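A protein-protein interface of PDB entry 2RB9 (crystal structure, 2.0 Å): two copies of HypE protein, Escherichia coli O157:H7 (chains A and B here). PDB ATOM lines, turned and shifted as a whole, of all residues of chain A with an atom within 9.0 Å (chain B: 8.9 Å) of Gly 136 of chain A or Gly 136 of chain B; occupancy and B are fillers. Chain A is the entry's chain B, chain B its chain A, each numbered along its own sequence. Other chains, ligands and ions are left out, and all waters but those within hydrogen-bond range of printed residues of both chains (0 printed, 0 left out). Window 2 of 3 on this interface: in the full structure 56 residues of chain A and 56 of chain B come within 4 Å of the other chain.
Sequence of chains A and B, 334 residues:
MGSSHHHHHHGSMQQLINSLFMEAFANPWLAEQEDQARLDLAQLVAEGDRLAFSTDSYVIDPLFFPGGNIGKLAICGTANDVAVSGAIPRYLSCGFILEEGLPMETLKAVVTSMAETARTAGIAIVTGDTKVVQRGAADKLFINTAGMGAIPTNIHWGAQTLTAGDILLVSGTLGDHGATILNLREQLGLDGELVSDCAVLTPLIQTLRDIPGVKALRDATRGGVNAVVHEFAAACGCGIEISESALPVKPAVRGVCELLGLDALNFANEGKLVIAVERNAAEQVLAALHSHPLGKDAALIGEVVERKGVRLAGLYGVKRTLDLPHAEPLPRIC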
ATOM      1  N   LEU A  98     -18.047 -23.392  -9.263  1.00  0.00           N
ATOM      2  CA  LEU A  98     -18.839 -24.189  -8.327  1.00  0.00           C
ATOM      3  C   LEU A  98     -19.629 -23.306  -7.371  1.00  0.00           C
ATOM      4  O   LEU A  98     -19.113 -22.297  -6.891  1.00  0.00           O
ATOM      5  CB  LEU A  98     -17.915 -25.098  -7.510  1.00  0.00           C
ATOM      6  CG  LEU A  98     -17.623 -26.547  -7.906  1.00  0.00           C
ATOM      7  CD1 LEU A  98     -17.340 -26.724  -9.388  1.00  0.00           C
ATOM      8  CD2 LEU A  98     -16.457 -27.053  -7.077  1.00  0.00           C
ATOM      9  N   GLU A  99     -20.867 -23.703  -7.090  1.00  0.00           N
ATOM     10  CA  GLU A  99     -21.687 -23.033  -6.085  1.00  0.00           C
ATOM     11  C   GLU A  99     -21.330 -23.623  -4.727  1.00  0.00           C
ATOM     12  O   GLU A  99     -21.305 -24.848  -4.566  1.00  0.00           O
ATOM     13  CB  GLU A  99     -23.173 -23.239  -6.374  1.00  0.00           C
ATOM     14  CG  GLU A  99     -24.107 -22.576  -5.364  1.00  0.00           C
ATOM     15  CD  GLU A  99     -25.583 -22.853  -5.636  1.00  0.00           C
ATOM     16  OE1 GLU A  99     -25.913 -23.916  -6.208  1.00  0.00           O
ATOM     17  OE2 GLU A  99     -26.417 -21.992  -5.281  1.00  0.00           O
ATOM     18  N   GLU A 100     -21.031 -22.758  -3.761  1.00  0.00           N
ATOM     19  CA  GLU A 100     -20.756 -23.198  -2.388  1.00  0.00           C
ATOM     20  C   GLU A 100     -21.902 -24.087  -1.901  1.00  0.00           C
ATOM     21  O   GLU A 100     -23.069 -23.746  -2.070  1.00  0.00           O
ATOM     22  CB  GLU A 100     -20.576 -21.985  -1.462  1.00  0.00           C
ATOM     23  CG  GLU A 100     -20.256 -22.315   0.002  1.00  0.00           C
ATOM     24  CD  GLU A 100     -18.823 -22.793   0.209  1.00  0.00           C
ATOM     25  OE1 GLU A 100     -17.890 -22.146  -0.319  1.00  0.00           O
ATOM     26  OE2 GLU A 100     -18.627 -23.816   0.908  1.00  0.00           O
ATOM     27  N   GLY A 101     -21.561 -25.237  -1.331  1.00  0.00           N
ATOM     28  CA  GLY A 101     -22.560 -26.154  -0.797  1.00  0.00           C
ATOM     29  C   GLY A 101     -22.979 -27.254  -1.754  1.00  0.00           C
ATOM     30  O   GLY A 101     -23.831 -28.081  -1.416  1.00  0.00           O
ATOM     31  N   VAL A 133     -18.195 -19.808  -5.860  1.00  0.00           N
ATOM     32  CA  VAL A 133     -19.009 -18.634  -5.587  1.00  0.00           C
ATOM     33  C   VAL A 133     -20.012 -18.990  -4.486  1.00  0.00           C
ATOM     34  O   VAL A 133     -20.211 -20.171  -4.187  1.00  0.00           O
ATOM     35  CB  VAL A 133     -19.712 -18.091  -6.867  1.00  0.00           C
ATOM     36  CG1 VAL A 133     -18.676 -17.725  -7.945  1.00  0.00           C
ATOM     37  CG2 VAL A 133     -20.705 -19.102  -7.425  1.00  0.00           C
ATOM     38  N   GLN A 134     -20.637 -17.983  -3.881  1.00  0.00           N
ATOM     39  CA  GLN A 134     -21.586 -18.233  -2.788  1.00  0.00           C
ATOM     40  C   GLN A 134     -22.895 -18.846  -3.289  1.00  0.00           C
ATOM     41  O   GLN A 134     -23.194 -18.797  -4.488  1.00  0.00           O
ATOM     42  CB  GLN A 134     -21.857 -16.963  -1.962  1.00  0.00           C
ATOM     43  CG  GLN A 134     -22.203 -15.718  -2.763  1.00  0.00           C
ATOM     44  CD  GLN A 134     -20.970 -15.016  -3.322  1.00  0.00           C
ATOM     45  OE1 GLN A 134     -19.991 -14.765  -2.608  1.00  0.00           O
ATOM     46  NE2 GLN A 134     -21.020 -14.690  -4.600  1.00  0.00           N
ATOM     47  N   ARG A 135     -23.655 -19.436  -2.366  1.00  0.00           N
ATOM     48  CA  ARG A 135     -24.995 -19.943  -2.661  1.00  0.00           C
ATOM     49  C   ARG A 135     -25.815 -18.875  -3.377  1.00  0.00           C
ATOM     50  O   ARG A 135     -25.849 -17.722  -2.950  1.00  0.00           O
ATOM     51  CB  ARG A 135     -25.711 -20.364  -1.371  1.00  0.00           C
ATOM     52  CG  ARG A 135     -25.223 -21.675  -0.781  1.00  0.00           C
ATOM     53  CD  ARG A 135     -25.822 -21.940   0.604  1.00  0.00           C
ATOM     54  NE  ARG A 135     -25.549 -23.301   1.072  1.00  0.00           N
ATOM     55  CZ  ARG A 135     -24.412 -23.691   1.647  1.00  0.00           C
ATOM     56  NH1 ARG A 135     -23.413 -22.831   1.830  1.00  0.00           N
ATOM     57  NH2 ARG A 135     -24.265 -24.951   2.037  1.00  0.00           N
ATOM     58  N   GLY A 136     -26.453 -19.258  -4.477  1.00  0.00           N
ATOM     59  CA  GLY A 136     -27.271 -18.331  -5.261  1.00  0.00           C
ATOM     60  C   GLY A 136     -26.547 -17.580  -6.370  1.00  0.00           C
ATOM     61  O   GLY A 136     -27.187 -17.045  -7.272  1.00  0.00           O
ATOM     62  N   ALA A 137     -25.218 -17.540  -6.308  1.00  0.00           N
ATOM     63  CA  ALA A 137     -24.415 -16.811  -7.299  1.00  0.00           C
ATOM     64  C   ALA A 137     -24.098 -17.627  -8.563  1.00  0.00           C
ATOM     65  O   ALA A 137     -23.648 -17.075  -9.564  1.00  0.00           O
ATOM     66  CB  ALA A 137     -23.141 -16.282  -6.665  1.00  0.00           C
ATOM     67  N   ALA A 138     -24.316 -18.938  -8.498  1.00  0.00           N
ATOM     68  CA  ALA A 138     -24.252 -19.816  -9.671  1.00  0.00           C
ATOM     69  C   ALA A 138     -25.123 -21.024  -9.401  1.00  0.00           C
ATOM     70  O   ALA A 138     -25.224 -21.465  -8.254  1.00  0.00           O
ATOM     71  CB  ALA A 138     -22.808 -20.261  -9.961  1.00  0.00           C
ATOM     72  N   ASP A 139     -25.749 -21.562 -10.446  1.00  0.00           N
ATOM     73  CA  ASP A 139     -26.614 -22.728 -10.285  1.00  0.00           C
ATOM     74  C   ASP A 139     -25.824 -24.039 -10.296  1.00  0.00           C
ATOM     75  O   ASP A 139     -25.704 -24.706 -11.337  1.00  0.00           O
ATOM     76  CB  ASP A 139     -27.731 -22.731 -11.338  1.00  0.00           C
ATOM     77  CG  ASP A 139     -28.709 -23.887 -11.161  1.00  0.00           C
ATOM     78  OD1 ASP A 139     -28.707 -24.537 -10.086  1.00  0.00           O
ATOM     79  OD2 ASP A 139     -29.473 -24.151 -12.112  1.00  0.00           O
ATOM     80  N   LYS A 140     -25.291 -24.393  -9.126  1.00  0.00           N
ATOM     81  CA  LYS A 140     -24.598 -25.668  -8.867  1.00  0.00           C
ATOM     82  C   LYS A 140     -23.191 -25.780  -9.452  1.00  0.00           C
ATOM     83  O   LYS A 140     -22.204 -25.783  -8.701  1.00  0.00           O
ATOM     84  CB  LYS A 140     -25.456 -26.885  -9.276  1.00  0.00           C
ATOM     85  CG  LYS A 140     -26.819 -26.969  -8.590  1.00  0.00           C
ATOM     86  CD  LYS A 140     -27.595 -28.197  -9.044  1.00  0.00           C
ATOM     87  CE  LYS A 140     -29.087 -28.066  -8.748  1.00  0.00           C
ATOM     88  NZ  LYS A 140     -29.766 -27.141  -9.709  1.00  0.00           N
ATOM     89  N   PHE A 142     -20.834 -24.972 -13.318  1.00  0.00           N
ATOM     90  CA  PHE A 142     -20.583 -24.658 -14.728  1.00  0.00           C
ATOM     91  C   PHE A 142     -19.164 -25.132 -15.052  1.00  0.00           C
ATOM     92  O   PHE A 142     -18.288 -25.092 -14.185  1.00  0.00           O
ATOM     93  CB  PHE A 142     -20.670 -23.155 -15.000  1.00  0.00           C
ATOM     94  CG  PHE A 142     -21.986 -22.522 -14.627  1.00  0.00           C
ATOM     95  CD1 PHE A 142     -23.199 -23.174 -14.865  1.00  0.00           C
ATOM     96  CD2 PHE A 142     -22.010 -21.244 -14.080  1.00  0.00           C
ATOM     97  CE1 PHE A 142     -24.415 -22.571 -14.531  1.00  0.00           C
ATOM     98  CE2 PHE A 142     -23.220 -20.634 -13.740  1.00  0.00           C
ATOM     99  CZ  PHE A 142     -24.425 -21.298 -13.976  1.00  0.00           C
ATOM    100  N   ARG A 332     -30.085 -23.368 -21.473  1.00  0.00           N
ATOM    101  CA  ARG A 332     -29.288 -24.381 -20.764  1.00  0.00           C
ATOM    102  C   ARG A 332     -29.549 -25.825 -21.213  1.00  0.00           C
ATOM    103  O   ARG A 332     -29.616 -26.751 -20.403  1.00  0.00           O
ATOM    104  CB  ARG A 332     -29.445 -24.213 -19.248  1.00  0.00           C
ATOM    105  CG  ARG A 332     -29.102 -22.796 -18.784  1.00  0.00           C
ATOM    106  CD  ARG A 332     -29.261 -22.633 -17.301  1.00  0.00           C
ATOM    107  NE  ARG A 332     -28.372 -23.511 -16.546  1.00  0.00           N
ATOM    108  CZ  ARG A 332     -28.466 -23.708 -15.237  1.00  0.00           C
ATOM    109  NH1 ARG A 332     -29.400 -23.075 -14.532  1.00  0.00           N
ATOM    110  NH2 ARG A 332     -27.631 -24.530 -14.632  1.00  0.00           N
ATOM    111  N   LEU B  98     -23.246 -15.544 -19.125  1.00  0.00           N
ATOM    112  CA  LEU B  98     -24.025 -14.316 -18.918  1.00  0.00           C
ATOM    113  C   LEU B  98     -25.354 -14.582 -18.224  1.00  0.00           C
ATOM    114  O   LEU B  98     -26.036 -15.558 -18.535  1.00  0.00           O
ATOM    115  CB  LEU B  98     -24.337 -13.661 -20.270  1.00  0.00           C
ATOM    116  CG  LEU B  98     -23.545 -12.476 -20.822  1.00  0.00           C
ATOM    117  CD1 LEU B  98     -22.071 -12.788 -20.951  1.00  0.00           C
ATOM    118  CD2 LEU B  98     -24.126 -12.081 -22.177  1.00  0.00           C
ATOM    119  N   GLU B  99     -25.733 -13.696 -17.309  1.00  0.00           N
ATOM    120  CA  GLU B  99     -27.043 -13.777 -16.688  1.00  0.00           C
ATOM    121  C   GLU B  99     -28.012 -13.020 -17.580  1.00  0.00           C
ATOM    122  O   GLU B  99     -27.761 -11.861 -17.940  1.00  0.00           O
ATOM    123  CB  GLU B  99     -27.026 -13.160 -15.291  1.00  0.00           C
ATOM    124  CG  GLU B  99     -28.342 -13.303 -14.532  1.00  0.00           C
ATOM    125  CD  GLU B  99     -28.331 -12.580 -13.183  1.00  0.00           C
ATOM    126  OE1 GLU B  99     -27.555 -11.610 -13.018  1.00  0.00           O
ATOM    127  OE2 GLU B  99     -29.099 -12.995 -12.286  1.00  0.00           O
ATOM    128  N   GLU B 100     -29.108 -13.678 -17.946  1.00  0.00           N
ATOM    129  CA  GLU B 100     -30.203 -13.015 -18.659  1.00  0.00           C
ATOM    130  C   GLU B 100     -30.547 -11.698 -17.967  1.00  0.00           C
ATOM    131  O   GLU B 100     -30.701 -11.651 -16.745  1.00  0.00           O
ATOM    132  CB  GLU B 100     -31.432 -13.929 -18.700  1.00  0.00           C
ATOM    133  CG  GLU B 100     -32.692 -13.309 -19.311  1.00  0.00           C
ATOM    134  CD  GLU B 100     -32.633 -13.196 -20.823  1.00  0.00           C
ATOM    135  OE1 GLU B 100     -32.353 -14.219 -21.492  1.00  0.00           O
ATOM    136  OE2 GLU B 100     -32.883 -12.083 -21.345  1.00  0.00           O
ATOM    137  N   GLY B 101     -30.636 -10.630 -18.750  1.00  0.00           N
ATOM    138  CA  GLY B 101     -31.001  -9.326 -18.221  1.00  0.00           C
ATOM    139  C   GLY B 101     -29.838  -8.415 -17.877  1.00  0.00           C
ATOM    140  O   GLY B 101     -30.052  -7.259 -17.512  1.00  0.00           O
ATOM    141  N   VAL B 133     -27.585 -17.810 -19.044  1.00  0.00           N
ATOM    142  CA  VAL B 133     -28.411 -18.522 -18.064  1.00  0.00           C
ATOM    143  C   VAL B 133     -29.530 -17.596 -17.583  1.00  0.00           C
ATOM    144  O   VAL B 133     -29.478 -16.392 -17.820  1.00  0.00           O
ATOM    145  CB  VAL B 133     -27.580 -19.098 -16.875  1.00  0.00           C
ATOM    146  CG1 VAL B 133     -26.524 -20.093 -17.380  1.00  0.00           C
ATOM    147  CG2 VAL B 133     -26.925 -17.987 -16.058  1.00  0.00           C
ATOM    148  N   GLN B 134     -30.552 -18.149 -16.935  1.00  0.00           N
ATOM    149  CA  GLN B 134     -31.675 -17.316 -16.500  1.00  0.00           C
ATOM    150  C   GLN B 134     -31.287 -16.429 -15.318  1.00  0.00           C
ATOM    151  O   GLN B 134     -30.263 -16.661 -14.673  1.00  0.00           O
ATOM    152  CB  GLN B 134     -32.924 -18.150 -16.176  1.00  0.00           C
ATOM    153  CG  GLN B 134     -32.704 -19.313 -15.223  1.00  0.00           C
ATOM    154  CD  GLN B 134     -32.164 -20.549 -15.926  1.00  0.00           C
ATOM    155  OE1 GLN B 134     -32.432 -20.783 -17.109  1.00  0.00           O
ATOM    156  NE2 GLN B 134     -31.404 -21.345 -15.200  1.00  0.00           N
ATOM    157  N   ARG B 135     -32.103 -15.408 -15.064  1.00  0.00           N
ATOM    158  CA  ARG B 135     -31.951 -14.551 -13.891  1.00  0.00           C
ATOM    159  C   ARG B 135     -31.796 -15.396 -12.631  1.00  0.00           C
ATOM    160  O   ARG B 135     -32.586 -16.306 -12.389  1.00  0.00           O
ATOM    161  CB  ARG B 135     -33.159 -13.620 -13.754  1.00  0.00           C
ATOM    162  CG  ARG B 135     -33.206 -12.520 -14.796  1.00  0.00           C
ATOM    163  CD  ARG B 135     -34.472 -11.674 -14.687  1.00  0.00           C
ATOM    164  NE  ARG B 135     -34.403 -10.483 -15.538  1.00  0.00           N
ATOM    165  CZ  ARG B 135     -34.669 -10.470 -16.843  1.00  0.00           C
ATOM    166  NH1 ARG B 135     -35.027 -11.587 -17.470  1.00  0.00           N
ATOM    167  NH2 ARG B 135     -34.570  -9.335 -17.526  1.00  0.00           N
ATOM    168  N   GLY B 136     -30.755 -15.112 -11.853  1.00  0.00           N
ATOM    169  CA  GLY B 136     -30.500 -15.843 -10.610  1.00  0.00           C
ATOM    170  C   GLY B 136     -29.592 -17.056 -10.733  1.00  0.00           C
ATOM    171  O   GLY B 136     -29.022 -17.494  -9.732  1.00  0.00           O
ATOM    172  N   ALA B 137     -29.453 -17.605 -11.945  1.00  0.00           N
ATOM    173  CA  ALA B 137     -28.587 -18.779 -12.172  1.00  0.00           C
ATOM    174  C   ALA B 137     -27.095 -18.440 -12.301  1.00  0.00           C
ATOM    175  O   ALA B 137     -26.244 -19.328 -12.233  1.00  0.00           O
ATOM    176  CB  ALA B 137     -29.066 -19.585 -13.374  1.00  0.00           C
ATOM    177  N   ALA B 138     -26.783 -17.164 -12.510  1.00  0.00           N
ATOM    178  CA  ALA B 138     -25.415 -16.659 -12.396  1.00  0.00           C
ATOM    179  C   ALA B 138     -25.452 -15.207 -11.949  1.00  0.00           C
ATOM    180  O   ALA B 138     -26.396 -14.485 -12.259  1.00  0.00           O
ATOM    181  CB  ALA B 138     -24.653 -16.790 -13.721  1.00  0.00           C
ATOM    182  N   ASP B 139     -24.428 -14.783 -11.216  1.00  0.00           N
ATOM    183  CA  ASP B 139     -24.355 -13.404 -10.757  1.00  0.00           C
ATOM    184  C   ASP B 139     -23.711 -12.534 -11.833  1.00  0.00           C
ATOM    185  O   ASP B 139     -22.503 -12.281 -11.811  1.00  0.00           O
ATOM    186  CB  ASP B 139     -23.601 -13.318  -9.419  1.00  0.00           C
ATOM    187  CG  ASP B 139     -23.585 -11.908  -8.833  1.00  0.00           C
ATOM    188  OD1 ASP B 139     -24.449 -11.080  -9.191  1.00  0.00           O
ATOM    189  OD2 ASP B 139     -22.695 -11.629  -8.005  1.00  0.00           O
ATOM    190  N   LYS B 140     -24.539 -12.101 -12.783  1.00  0.00           N
ATOM    191  CA  LYS B 140     -24.174 -11.135 -13.827  1.00  0.00           C
ATOM    192  C   LYS B 140     -23.327 -11.685 -14.981  1.00  0.00           C
ATOM    193  O   LYS B 140     -23.830 -11.838 -16.099  1.00  0.00           O
ATOM    194  CB  LYS B 140     -23.521  -9.865 -13.247  1.00  0.00           C
ATOM    195  CG  LYS B 140     -24.396  -9.072 -12.277  1.00  0.00           C
ATOM    196  CD  LYS B 140     -23.653  -7.853 -11.743  1.00  0.00           C
ATOM    197  CE  LYS B 140     -24.331  -7.272 -10.505  1.00  0.00           C
ATOM    198  NZ  LYS B 140     -24.260  -8.212  -9.353  1.00  0.00           N
ATOM    199  N   PHE B 142     -19.593 -14.231 -15.753  1.00  0.00           N
ATOM    200  CA  PHE B 142     -18.364 -14.987 -15.470  1.00  0.00           C
ATOM    201  C   PHE B 142     -17.598 -15.178 -16.780  1.00  0.00           C
ATOM    202  O   PHE B 142     -18.210 -15.309 -17.845  1.00  0.00           O
ATOM    203  CB  PHE B 142     -18.655 -16.374 -14.873  1.00  0.00           C
ATOM    204  CG  PHE B 142     -19.471 -16.356 -13.601  1.00  0.00           C
ATOM    205  CD1 PHE B 142     -19.294 -15.356 -12.639  1.00  0.00           C
ATOM    206  CD2 PHE B 142     -20.390 -17.371 -13.352  1.00  0.00           C
ATOM    207  CE1 PHE B 142     -20.048 -15.355 -11.455  1.00  0.00           C
ATOM    208  CE2 PHE B 142     -21.147 -17.385 -12.183  1.00  0.00           C
ATOM    209  CZ  PHE B 142     -20.975 -16.375 -11.227  1.00  0.00           C
ATOM    210  N   ARG B 332     -14.596 -14.403  -4.276  1.00  0.00           N
ATOM    211  CA  ARG B 332     -14.713 -13.643  -5.527  1.00  0.00           C
ATOM    212  C   ARG B 332     -13.887 -12.349  -5.575  1.00  0.00           C
ATOM    213  O   ARG B 332     -14.375 -11.289  -5.980  1.00  0.00           O
ATOM    214  CB  ARG B 332     -16.192 -13.395  -5.869  1.00  0.00           C
ATOM    215  CG  ARG B 332     -16.984 -14.701  -6.005  1.00  0.00           C
ATOM    216  CD  ARG B 332     -18.452 -14.468  -6.296  1.00  0.00           C
ATOM    217  NE  ARG B 332     -18.673 -13.701  -7.518  1.00  0.00           N
ATOM    218  CZ  ARG B 332     -19.842 -13.163  -7.854  1.00  0.00           C
ATOM    219  NH1 ARG B 332     -20.900 -13.315  -7.065  1.00  0.00           N
ATOM    220  NH2 ARG B 332     -19.954 -12.464  -8.972  1.00  0.00           N
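The side-chain carboxylate (OE2) of Glu 99 of chain B sits at hydrogen-bond distance from the backbone NH (N) of Gly 136 of chain B, 2.7 Å away. The side-chain amino group (NZ) of Lys 140 of chain B is in salt-bridge range of the side-chain carboxylate (OD1) of Asp 139 of chain B (2.9 Å). The side-chain carboxylate of Asp 139 of chain B lies within salt-bridge range of the guanidinium group of Arg 332 of chain B (2.6 Å). The backbone NH of Gly 136 of chain A is in hydrogen-bond range of the side-chain carboxylate of Glu 99 of chain A, at 2.8 Å. NZ of Lys 140 of chain A is in salt-bridge range of OD1 of Asp 139 of chain A, 2.8 Å away. OD2 of Asp 139 of chain A lies within salt-bridge range of NH1 of Arg 332 of chain A, 2.6 Å away.
Gly 136 of chain B touches just one residue of chain A: Gly 136. Of chain B, only Ala 138, Asp 139, Phe 142 and Arg 332 come within 4 Å of Ala 137 of chain A. Ala 137 of chain B touches just these residues of chain A: Ala 138 (3.3 Å), Asp 139 (2.9 Å), Phe 142 (3.2 Å) and Arg 332 (3.7 Å). Of the printed residues of chain B, Val 133 of chain A touches Arg 332. Of the printed residues of chain A, Ala 138 of chain B touches Ala 137 (3.4 Å). Of the printed residues of chain B, Arg 332 of chain A touches Val 133, Gln 134 and Ala 137. Glu 99 of chain A touches none of the printed residues of chain B. The nearest printed residue of chain A that does not touch Gly 136 of chain B is Ala 137 of chain A (5.1 Å). The nearest printed residue of chain A that does not touch Arg 332 of chain B is Ala 138 of chain A (6.7 Å).
Among the printed residues, pairs that only touch across the chains: Val 133 of chain A with Arg 332 of chain B (3.7 Å), Ala 137 of chain A with Ala 138 of chain B (3.4 Å), Ala 137 of chain A with Phe 142 of chain B (3.2 Å), Ala 137 of chain A with Arg 332 of chain B (3.7 Å), Ala 138 of chain A with Ala 137 of chain B (3.3 Å), Ala 138 of chain A with Phe 142 of chain B (3.996 Å), Phe 142 of chain A with Ala 137 of chain B (3.2 Å), Arg 332 of chain A with Val 133 of chain B (3.7 Å) and Arg 332 of chain A with Ala 137 of chain B (3.7 Å).
Hydrophobic or aromatic side chains of chain B within 4 Å of the printed part of chain A: Val 133, Ala 137 and Phe 142. Of the 14 printed residues of chain A, 8 touch a printed residue of chain B. Hydrophobic or aromatic side chains of chain A that line the printed part of chain B: Val 133, Ala 137, Ala 138 and Phe 142. Among the printed residues, 14 pairs touch across the chains. Among the printed residues, no Asp or Glu carboxylate lies within 4 Å of a Lys or Arg side-chain nitrogen of the other chain.
Gly 136 of chain B touches its own counterpart, Gly 136 of chain A. Ala 137 of chain A touches Ala 138 of chain B, and with the chains exchanged Ala 138 of chain A touches Ala 137 of chain B. Ala 137 of chain A touches Arg 332 of chain B, and with the chains exchanged Arg 332 of chain A touches Ala 137 of chain B. Ala 138 of chain A touches Phe 142 of chain B, but with the chains exchanged Phe 142 of chain A does not touch Ala 138 of chain B (4.1 Å). 14 positions are printed for both chains. Of the 14 pairs that touch across the chains among the printed residues, 13 have their exchanged pair printed and touching as well.
The guanidinium group (NH1) of Arg 332 of chain A sits close to the side-chain amide nitrogen (NE2) of Gln 134 of chain B. The backbone NH (N) of Asp 139 of chain A sits at hydrogen-bond distance from the backbone carbonyl oxygen (O) of Ala 137 of chain B. N of Asp 139 of chain B is in hydrogen-bond range of O of Ala 137 of chain A, 2.9 Å away. NH1 of Arg 332 of chain B lies close to NE2 of Gln 134 of chain A, at 2.8 Å. O of Gly 136 of chain B lies close to O of Gly 136 of chain A, 3.1 Å away.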
